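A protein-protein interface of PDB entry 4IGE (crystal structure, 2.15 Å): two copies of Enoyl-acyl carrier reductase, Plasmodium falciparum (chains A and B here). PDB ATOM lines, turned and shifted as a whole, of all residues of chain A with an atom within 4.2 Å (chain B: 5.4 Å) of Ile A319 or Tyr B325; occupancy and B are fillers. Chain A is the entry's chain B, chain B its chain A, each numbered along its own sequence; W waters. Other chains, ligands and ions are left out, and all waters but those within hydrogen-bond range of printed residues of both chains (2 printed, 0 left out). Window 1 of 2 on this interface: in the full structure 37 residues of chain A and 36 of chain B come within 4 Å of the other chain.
N of Asp B327 lies within hydrogen-bond range of O of Ala A318 (3.1 Å).
The backbone NH of Asn B328 sits at hydrogen-bond distance from the backbone carbonyl oxygen of Ala A318 (2.8 Å).
ND2 of Asn B331 sits close to NE2 of Gln A322 (3.3 Å).
Printed residues of chain B within 4 Å of Ile A319: Val B307 (3.7 Å) and Tyr B325 (3.7 Å).
Gln B184 touches none of the printed residues of chain A.
Thr B323 touches none of the printed residues of chain A.
Tyr B325 touches two residues of chain A.
Printed residues of chain A within 4 Å of Val B326: Ala A318 (3.7 Å).
Of the printed residues of chain A, Asn B328 touches Ala A318 and Thr A320.
Of the printed residues of chain A, Asn B331 touches Gln A322 (3.3 Å).
CG of Arg A219 touches CD1 of Leu B295 (3.7 Å).
Phe A310 touches Val B307.
Arg A317 touches Leu B295 (O to CD1, 3.4 Å).
Val B326 touches Ala A318.
CG2 of Val B307 touches CD1 of Ile A319 (3.7 Å).
Ile A319 touches Tyr B325 (CG1 to O, 3.7 Å).
CG2 of Thr A320 touches CD1 of Leu B295, 3.9 Å away.
O of Asn B328 touches CG2 of Thr A320, at 3.9 Å.
OE1 of Gln A322 touches CB of Tyr B325, 3.4 Å away.
Printed residues of chain A that touch a printed residue of chain B: Arg A219, Phe A310, Arg A317, Ala A318, Ile A319, Thr A320 and Gln A322.
Hydrophobic or aromatic side chains of chain A that line the printed part of chain B: Phe A310, Ala A318 and Ile A319.
Hydrophobic or aromatic side chains of chain B that line the printed part of chain A: Leu B295, Val B307, Tyr B325 and Val B326.
Among the printed residues, no Asp or Glu carboxylate lies within 4 Å of a Lys or Arg side-chain nitrogen of the other chain.
No position is printed for both chains.
N of Val B326 lies within hydrogen-bond range of O of Ser B224, at 2.9 Å.
The side-chain carboxylate (OD2) of Asp B327 sits at hydrogen-bond distance from the side-chain amide nitrogen (ND2) of Asn B331.
The backbone carbonyl oxygen of Ile A319 is in hydrogen-bond range of the guanidinium group of Arg A219, at 3.0 Å.
The side-chain amide oxygen of Asn A221 lies within hydrogen-bond range of the backbone NH of Gln A322, 2.9 Å away.
OG of Ser A316 sits at hydrogen-bond distance from O of Phe A310 (3.1 Å).
The backbone carbonyl oxygen (O) of Thr A320 is in hydrogen-bond range of the side-chain amide nitrogen (NE2) of Gln A322 (3.1 Å).
Water W1 lies within hydrogen-bond range of the backbone carbonyl oxygen of Tyr B325, the side-chain carboxylate of Asp B327 and the backbone NH of Thr A320.
Water W2 lies within hydrogen-bond range of the side-chain amide oxygen of Gln A322 and the backbone NH of Tyr B325.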
ATOM      1  N   ARG A 219     -15.693  13.548  13.472  1.00  0.00           N
ATOM      2  CA  ARG A 219     -16.802  13.982  12.621  1.00  0.00           C
ATOM      3  C   ARG A 219     -18.144  13.621  13.259  1.00  0.00           C
ATOM      4  O   ARG A 219     -18.238  12.658  14.036  1.00  0.00           O
ATOM      5  CB  ARG A 219     -16.695  13.321  11.251  1.00  0.00           C
ATOM      6  CG  ARG A 219     -15.472  13.745  10.451  1.00  0.00           C
ATOM      7  CD  ARG A 219     -15.532  13.185   9.035  1.00  0.00           C
ATOM      8  NE  ARG A 219     -15.466  11.729   9.037  1.00  0.00           N
ATOM      9  CZ  ARG A 219     -16.470  10.921   8.717  1.00  0.00           C
ATOM     10  NH1 ARG A 219     -17.656  11.405   8.343  1.00  0.00           N
ATOM     11  NH2 ARG A 219     -16.281   9.618   8.757  1.00  0.00           N
ATOM     12  N   ASN A 221     -22.510  13.585  12.092  1.00  0.00           N
ATOM     13  CA  ASN A 221     -23.600  13.842  11.172  1.00  0.00           C
ATOM     14  C   ASN A 221     -24.900  13.272  11.725  1.00  0.00           C
ATOM     15  O   ASN A 221     -24.906  12.543  12.738  1.00  0.00           O
ATOM     16  CB  ASN A 221     -23.293  13.224   9.800  1.00  0.00           C
ATOM     17  CG  ASN A 221     -22.074  13.870   9.125  1.00  0.00           C
ATOM     18  OD1 ASN A 221     -22.143  14.992   8.610  1.00  0.00           O
ATOM     19  ND2 ASN A 221     -20.958  13.159   9.134  1.00  0.00           N
ATOM     20  N   PHE A 310     -21.572   3.884   6.133  1.00  0.00           N
ATOM     21  CA  PHE A 310     -20.778   4.720   5.271  1.00  0.00           C
ATOM     22  C   PHE A 310     -20.286   5.965   6.027  1.00  0.00           C
ATOM     23  O   PHE A 310     -19.101   6.292   5.986  1.00  0.00           O
ATOM     24  CB  PHE A 310     -21.601   5.092   4.044  1.00  0.00           C
ATOM     25  CG  PHE A 310     -21.078   6.278   3.308  1.00  0.00           C
ATOM     26  CD1 PHE A 310     -19.905   6.195   2.583  1.00  0.00           C
ATOM     27  CD2 PHE A 310     -21.751   7.479   3.349  1.00  0.00           C
ATOM     28  CE1 PHE A 310     -19.415   7.293   1.909  1.00  0.00           C
ATOM     29  CE2 PHE A 310     -21.273   8.583   2.678  1.00  0.00           C
ATOM     30  CZ  PHE A 310     -20.103   8.494   1.961  1.00  0.00           C
ATOM     31  N   SER A 316     -16.252   8.629   4.223  1.00  0.00           N
ATOM     32  CA  SER A 316     -17.002   9.875   4.320  1.00  0.00           C
ATOM     33  C   SER A 316     -16.207  10.958   5.067  1.00  0.00           C
ATOM     34  O   SER A 316     -16.781  11.884   5.635  1.00  0.00           O
ATOM     35  CB  SER A 316     -18.332   9.613   5.038  1.00  0.00           C
ATOM     36  OG  SER A 316     -18.119   9.161   6.371  1.00  0.00           O
ATOM     37  N   ARG A 317     -14.881  10.839   5.060  1.00  0.00           N
ATOM     38  CA  ARG A 317     -14.021  11.727   5.847  1.00  0.00           C
ATOM     39  C   ARG A 317     -14.179  13.237   5.578  1.00  0.00           C
ATOM     40  O   ARG A 317     -13.829  14.044   6.426  1.00  0.00           O
ATOM     41  CB  ARG A 317     -12.533  11.325   5.667  1.00  0.00           C
ATOM     42  CG  ARG A 317     -12.072  11.458   4.228  1.00  0.00           C
ATOM     43  CD  ARG A 317     -10.578  11.081   4.021  1.00  0.00           C
ATOM     44  NE  ARG A 317      -9.667  11.750   4.950  1.00  0.00           N
ATOM     45  CZ  ARG A 317      -8.803  12.722   4.637  1.00  0.00           C
ATOM     46  NH1 ARG A 317      -8.702  13.194   3.393  1.00  0.00           N
ATOM     47  NH2 ARG A 317      -8.025  13.227   5.591  1.00  0.00           N
ATOM     48  N   ALA A 318     -14.652  13.639   4.399  1.00  0.00           N
ATOM     49  CA  ALA A 318     -14.872  15.067   4.164  1.00  0.00           C
ATOM     50  C   ALA A 318     -16.314  15.538   4.427  1.00  0.00           C
ATOM     51  O   ALA A 318     -16.685  16.672   4.070  1.00  0.00           O
ATOM     52  CB  ALA A 318     -14.411  15.473   2.750  1.00  0.00           C
ATOM     53  N   ILE A 319     -17.110  14.682   5.062  1.00  0.00           N
ATOM     54  CA  ILE A 319     -18.496  15.016   5.398  1.00  0.00           C
ATOM     55  C   ILE A 319     -18.704  15.190   6.905  1.00  0.00           C
ATOM     56  O   ILE A 319     -18.504  14.248   7.668  1.00  0.00           O
ATOM     57  CB  ILE A 319     -19.494  13.914   4.933  1.00  0.00           C
ATOM     58  CG1 ILE A 319     -19.408  13.678   3.421  1.00  0.00           C
ATOM     59  CG2 ILE A 319     -20.933  14.327   5.296  1.00  0.00           C
ATOM     60  CD1 ILE A 319     -20.374  12.585   2.921  1.00  0.00           C
ATOM     61  N   THR A 320     -19.134  16.370   7.346  1.00  0.00           N
ATOM     62  CA  THR A 320     -19.434  16.533   8.765  1.00  0.00           C
ATOM     63  C   THR A 320     -20.468  17.639   8.986  1.00  0.00           C
ATOM     64  O   THR A 320     -20.547  18.572   8.189  1.00  0.00           O
ATOM     65  CB  THR A 320     -18.152  16.771   9.602  1.00  0.00           C
ATOM     66  OG1 THR A 320     -18.447  16.599  10.985  1.00  0.00           O
ATOM     67  CG2 THR A 320     -17.552  18.161   9.349  1.00  0.00           C
ATOM     68  N   GLN A 322     -23.670  17.411   8.757  1.00  0.00           N
ATOM     69  CA  GLN A 322     -24.717  17.316   7.759  1.00  0.00           C
ATOM     70  C   GLN A 322     -25.962  16.571   8.237  1.00  0.00           C
ATOM     71  O   GLN A 322     -25.894  15.648   9.050  1.00  0.00           O
ATOM     72  CB  GLN A 322     -24.158  16.603   6.533  1.00  0.00           C
ATOM     73  CG  GLN A 322     -22.999  17.347   5.887  1.00  0.00           C
ATOM     74  CD  GLN A 322     -23.376  18.774   5.603  1.00  0.00           C
ATOM     75  OE1 GLN A 322     -24.248  19.021   4.785  1.00  0.00           O
ATOM     76  NE2 GLN A 322     -22.781  19.721   6.342  1.00  0.00           N
ATOM     77  N   HIS B 181     -21.699  25.430  -3.554  1.00  0.00           N
ATOM     78  CA  HIS B 181     -22.544  26.125  -2.576  1.00  0.00           C
ATOM     79  C   HIS B 181     -22.877  27.568  -3.006  1.00  0.00           C
ATOM     80  O   HIS B 181     -23.727  28.214  -2.402  1.00  0.00           O
ATOM     81  CB  HIS B 181     -21.822  26.116  -1.215  1.00  0.00           C
ATOM     82  CG  HIS B 181     -22.655  26.556  -0.037  1.00  0.00           C
ATOM     83  ND1 HIS B 181     -23.856  25.964   0.303  1.00  0.00           N
ATOM     84  CD2 HIS B 181     -22.409  27.479   0.928  1.00  0.00           C
ATOM     85  CE1 HIS B 181     -24.329  26.522   1.405  1.00  0.00           C
ATOM     86  NE2 HIS B 181     -23.464  27.438   1.810  1.00  0.00           N
ATOM     87  N   SER B 183     -24.627  28.362  -5.346  1.00  0.00           N
ATOM     88  CA  SER B 183     -26.046  28.268  -5.689  1.00  0.00           C
ATOM     89  C   SER B 183     -26.950  28.759  -4.533  1.00  0.00           C
ATOM     90  O   SER B 183     -28.013  29.340  -4.747  1.00  0.00           O
ATOM     91  CB  SER B 183     -26.385  26.804  -5.984  1.00  0.00           C
ATOM     92  OG  SER B 183     -26.162  26.028  -4.810  1.00  0.00           O
ATOM     93  N   GLN B 184     -26.510  28.509  -3.306  1.00  0.00           N
ATOM     94  CA  GLN B 184     -27.338  28.716  -2.128  1.00  0.00           C
ATOM     95  C   GLN B 184     -26.934  29.959  -1.330  1.00  0.00           C
ATOM     96  O   GLN B 184     -27.770  30.562  -0.654  1.00  0.00           O
ATOM     97  CB  GLN B 184     -27.276  27.468  -1.229  1.00  0.00           C
ATOM     98  CG  GLN B 184     -27.788  26.208  -1.890  1.00  0.00           C
ATOM     99  CD  GLN B 184     -29.219  26.382  -2.371  1.00  0.00           C
ATOM    100  OE1 GLN B 184     -30.036  27.006  -1.691  1.00  0.00           O
ATOM    101  NE2 GLN B 184     -29.528  25.843  -3.550  1.00  0.00           N
ATOM    102  N   GLU B 202     -29.220  21.735  -8.886  1.00  0.00           N
ATOM    103  CA  GLU B 202     -29.709  21.169  -7.628  1.00  0.00           C
ATOM    104  C   GLU B 202     -31.239  20.976  -7.613  1.00  0.00           C
ATOM    105  O   GLU B 202     -31.770  19.994  -7.054  1.00  0.00           O
ATOM    106  CB  GLU B 202     -29.246  22.038  -6.447  1.00  0.00           C
ATOM    107  CG  GLU B 202     -27.736  21.975  -6.217  1.00  0.00           C
ATOM    108  CD  GLU B 202     -27.206  23.010  -5.202  1.00  0.00           C
ATOM    109  OE1 GLU B 202     -27.908  23.357  -4.227  1.00  0.00           O
ATOM    110  OE2 GLU B 202     -26.070  23.473  -5.391  1.00  0.00           O
ATOM    111  N   SER B 224     -22.256  18.459  -3.560  1.00  0.00           N
ATOM    112  CA  SER B 224     -21.746  19.798  -3.450  1.00  0.00           C
ATOM    113  C   SER B 224     -20.326  19.769  -2.858  1.00  0.00           C
ATOM    114  O   SER B 224     -20.132  19.584  -1.655  1.00  0.00           O
ATOM    115  CB  SER B 224     -22.705  20.687  -2.628  1.00  0.00           C
ATOM    116  OG  SER B 224     -22.306  22.041  -2.747  1.00  0.00           O
ATOM    117  N   LEU B 295     -13.201  20.767   9.638  1.00  0.00           N
ATOM    118  CA  LEU B 295     -12.106  19.820   9.489  1.00  0.00           C
ATOM    119  C   LEU B 295     -11.016  20.496   8.697  1.00  0.00           C
ATOM    120  O   LEU B 295     -11.239  20.942   7.561  1.00  0.00           O
ATOM    121  CB  LEU B 295     -12.558  18.560   8.748  1.00  0.00           C
ATOM    122  CG  LEU B 295     -13.681  17.808   9.464  1.00  0.00           C
ATOM    123  CD1 LEU B 295     -14.073  16.597   8.651  1.00  0.00           C
ATOM    124  CD2 LEU B 295     -13.221  17.401  10.845  1.00  0.00           C
ATOM    125  N   VAL B 307     -17.267   9.424  -1.845  1.00  0.00           N
ATOM    126  CA  VAL B 307     -18.673   9.724  -1.598  1.00  0.00           C
ATOM    127  C   VAL B 307     -19.455   9.360  -2.850  1.00  0.00           C
ATOM    128  O   VAL B 307     -20.506   8.712  -2.753  1.00  0.00           O
ATOM    129  CB  VAL B 307     -18.894  11.175  -1.154  1.00  0.00           C
ATOM    130  CG1 VAL B 307     -20.409  11.483  -1.005  1.00  0.00           C
ATOM    131  CG2 VAL B 307     -18.152  11.398   0.147  1.00  0.00           C
ATOM    132  N   THR B 323     -28.799  16.856  -2.343  1.00  0.00           N
ATOM    133  CA  THR B 323     -27.530  17.557  -2.475  1.00  0.00           C
ATOM    134  C   THR B 323     -26.695  17.191  -1.267  1.00  0.00           C
ATOM    135  O   THR B 323     -27.048  17.531  -0.131  1.00  0.00           O
ATOM    136  CB  THR B 323     -27.725  19.065  -2.495  1.00  0.00           C
ATOM    137  OG1 THR B 323     -28.471  19.421  -3.665  1.00  0.00           O
ATOM    138  CG2 THR B 323     -26.348  19.804  -2.478  1.00  0.00           C
ATOM    139  N   ILE B 324     -25.600  16.472  -1.492  1.00  0.00           N
ATOM    140  CA  ILE B 324     -24.776  15.983  -0.383  1.00  0.00           C
ATOM    141  C   ILE B 324     -23.504  16.820  -0.314  1.00  0.00           C
ATOM    142  O   ILE B 324     -22.762  16.862  -1.277  1.00  0.00           O
ATOM    143  CB  ILE B 324     -24.389  14.492  -0.570  1.00  0.00           C
ATOM    144  CG1 ILE B 324     -25.637  13.605  -0.774  1.00  0.00           C
ATOM    145  CG2 ILE B 324     -23.473  13.988   0.575  1.00  0.00           C
ATOM    146  CD1 ILE B 324     -26.570  13.490   0.407  1.00  0.00           C
ATOM    147  N   TYR B 325     -23.254  17.480   0.821  1.00  0.00           N
ATOM    148  CA  TYR B 325     -22.092  18.343   0.956  1.00  0.00           C
ATOM    149  C   TYR B 325     -20.822  17.571   1.330  1.00  0.00           C
ATOM    150  O   TYR B 325     -20.757  16.914   2.368  1.00  0.00           O
ATOM    151  CB  TYR B 325     -22.355  19.450   1.977  1.00  0.00           C
ATOM    152  CG  TYR B 325     -23.168  20.594   1.385  1.00  0.00           C
ATOM    153  CD1 TYR B 325     -24.558  20.504   1.231  1.00  0.00           C
ATOM    154  CD2 TYR B 325     -22.539  21.747   0.964  1.00  0.00           C
ATOM    155  CE1 TYR B 325     -25.298  21.581   0.667  1.00  0.00           C
ATOM    156  CE2 TYR B 325     -23.234  22.797   0.414  1.00  0.00           C
ATOM    157  CZ  TYR B 325     -24.604  22.727   0.265  1.00  0.00           C
ATOM    158  OH  TYR B 325     -25.229  23.827  -0.304  1.00  0.00           O
ATOM    159  N   VAL B 326     -19.806  17.663   0.477  1.00  0.00           N
ATOM    160  CA  VAL B 326     -18.536  16.981   0.747  1.00  0.00           C
ATOM    161  C   VAL B 326     -17.482  18.049   0.671  1.00  0.00           C
ATOM    162  O   VAL B 326     -16.930  18.295  -0.403  1.00  0.00           O
ATOM    163  CB  VAL B 326     -18.256  15.877  -0.299  1.00  0.00           C
ATOM    164  CG1 VAL B 326     -16.974  15.119   0.049  1.00  0.00           C
ATOM    165  CG2 VAL B 326     -19.483  14.912  -0.411  1.00  0.00           C
ATOM    166  N   ASP B 327     -17.244  18.714   1.798  1.00  0.00           N
ATOM    167  CA  ASP B 327     -16.537  20.002   1.813  1.00  0.00           C
ATOM    168  C   ASP B 327     -15.887  20.275   3.148  1.00  0.00           C
ATOM    169  O   ASP B 327     -15.739  21.448   3.533  1.00  0.00           O
ATOM    170  CB  ASP B 327     -17.526  21.150   1.539  1.00  0.00           C
ATOM    171  CG  ASP B 327     -18.590  21.312   2.664  1.00  0.00           C
ATOM    172  OD1 ASP B 327     -18.742  20.410   3.532  1.00  0.00           O
ATOM    173  OD2 ASP B 327     -19.306  22.332   2.659  1.00  0.00           O
ATOM    174  N   ASN B 328     -15.555  19.211   3.884  1.00  0.00           N
ATOM    175  CA  ASN B 328     -14.985  19.366   5.228  1.00  0.00           C
ATOM    176  C   ASN B 328     -15.845  20.154   6.210  1.00  0.00           C
ATOM    177  O   ASN B 328     -15.361  20.607   7.257  1.00  0.00           O
ATOM    178  CB  ASN B 328     -13.577  19.956   5.153  1.00  0.00           C
ATOM    179  CG  ASN B 328     -12.583  18.969   4.587  1.00  0.00           C
ATOM    180  OD1 ASN B 328     -12.780  17.761   4.691  1.00  0.00           O
ATOM    181  ND2 ASN B 328     -11.534  19.470   3.958  1.00  0.00           N
ATOM    182  N   ASN B 331     -19.764  24.440   4.658  1.00  0.00           N
ATOM    183  CA  ASN B 331     -21.085  25.021   4.415  1.00  0.00           C
ATOM    184  C   ASN B 331     -21.856  25.351   5.703  1.00  0.00           C
ATOM    185  O   ASN B 331     -22.792  26.155   5.685  1.00  0.00           O
ATOM    186  CB  ASN B 331     -21.932  24.077   3.561  1.00  0.00           C
ATOM    187  CG  ASN B 331     -22.283  22.780   4.303  1.00  0.00           C
ATOM    188  OD1 ASN B 331     -23.308  22.697   4.970  1.00  0.00           O
ATOM    189  ND2 ASN B 331     -21.400  21.790   4.226  1.00  0.00           N
HETATM  190  O   HOH W   1     -20.103  18.126   4.715  1.00  0.00           O
HETATM  191  O   HOH W   2     -25.125  17.113   2.943  1.00  0.00           O
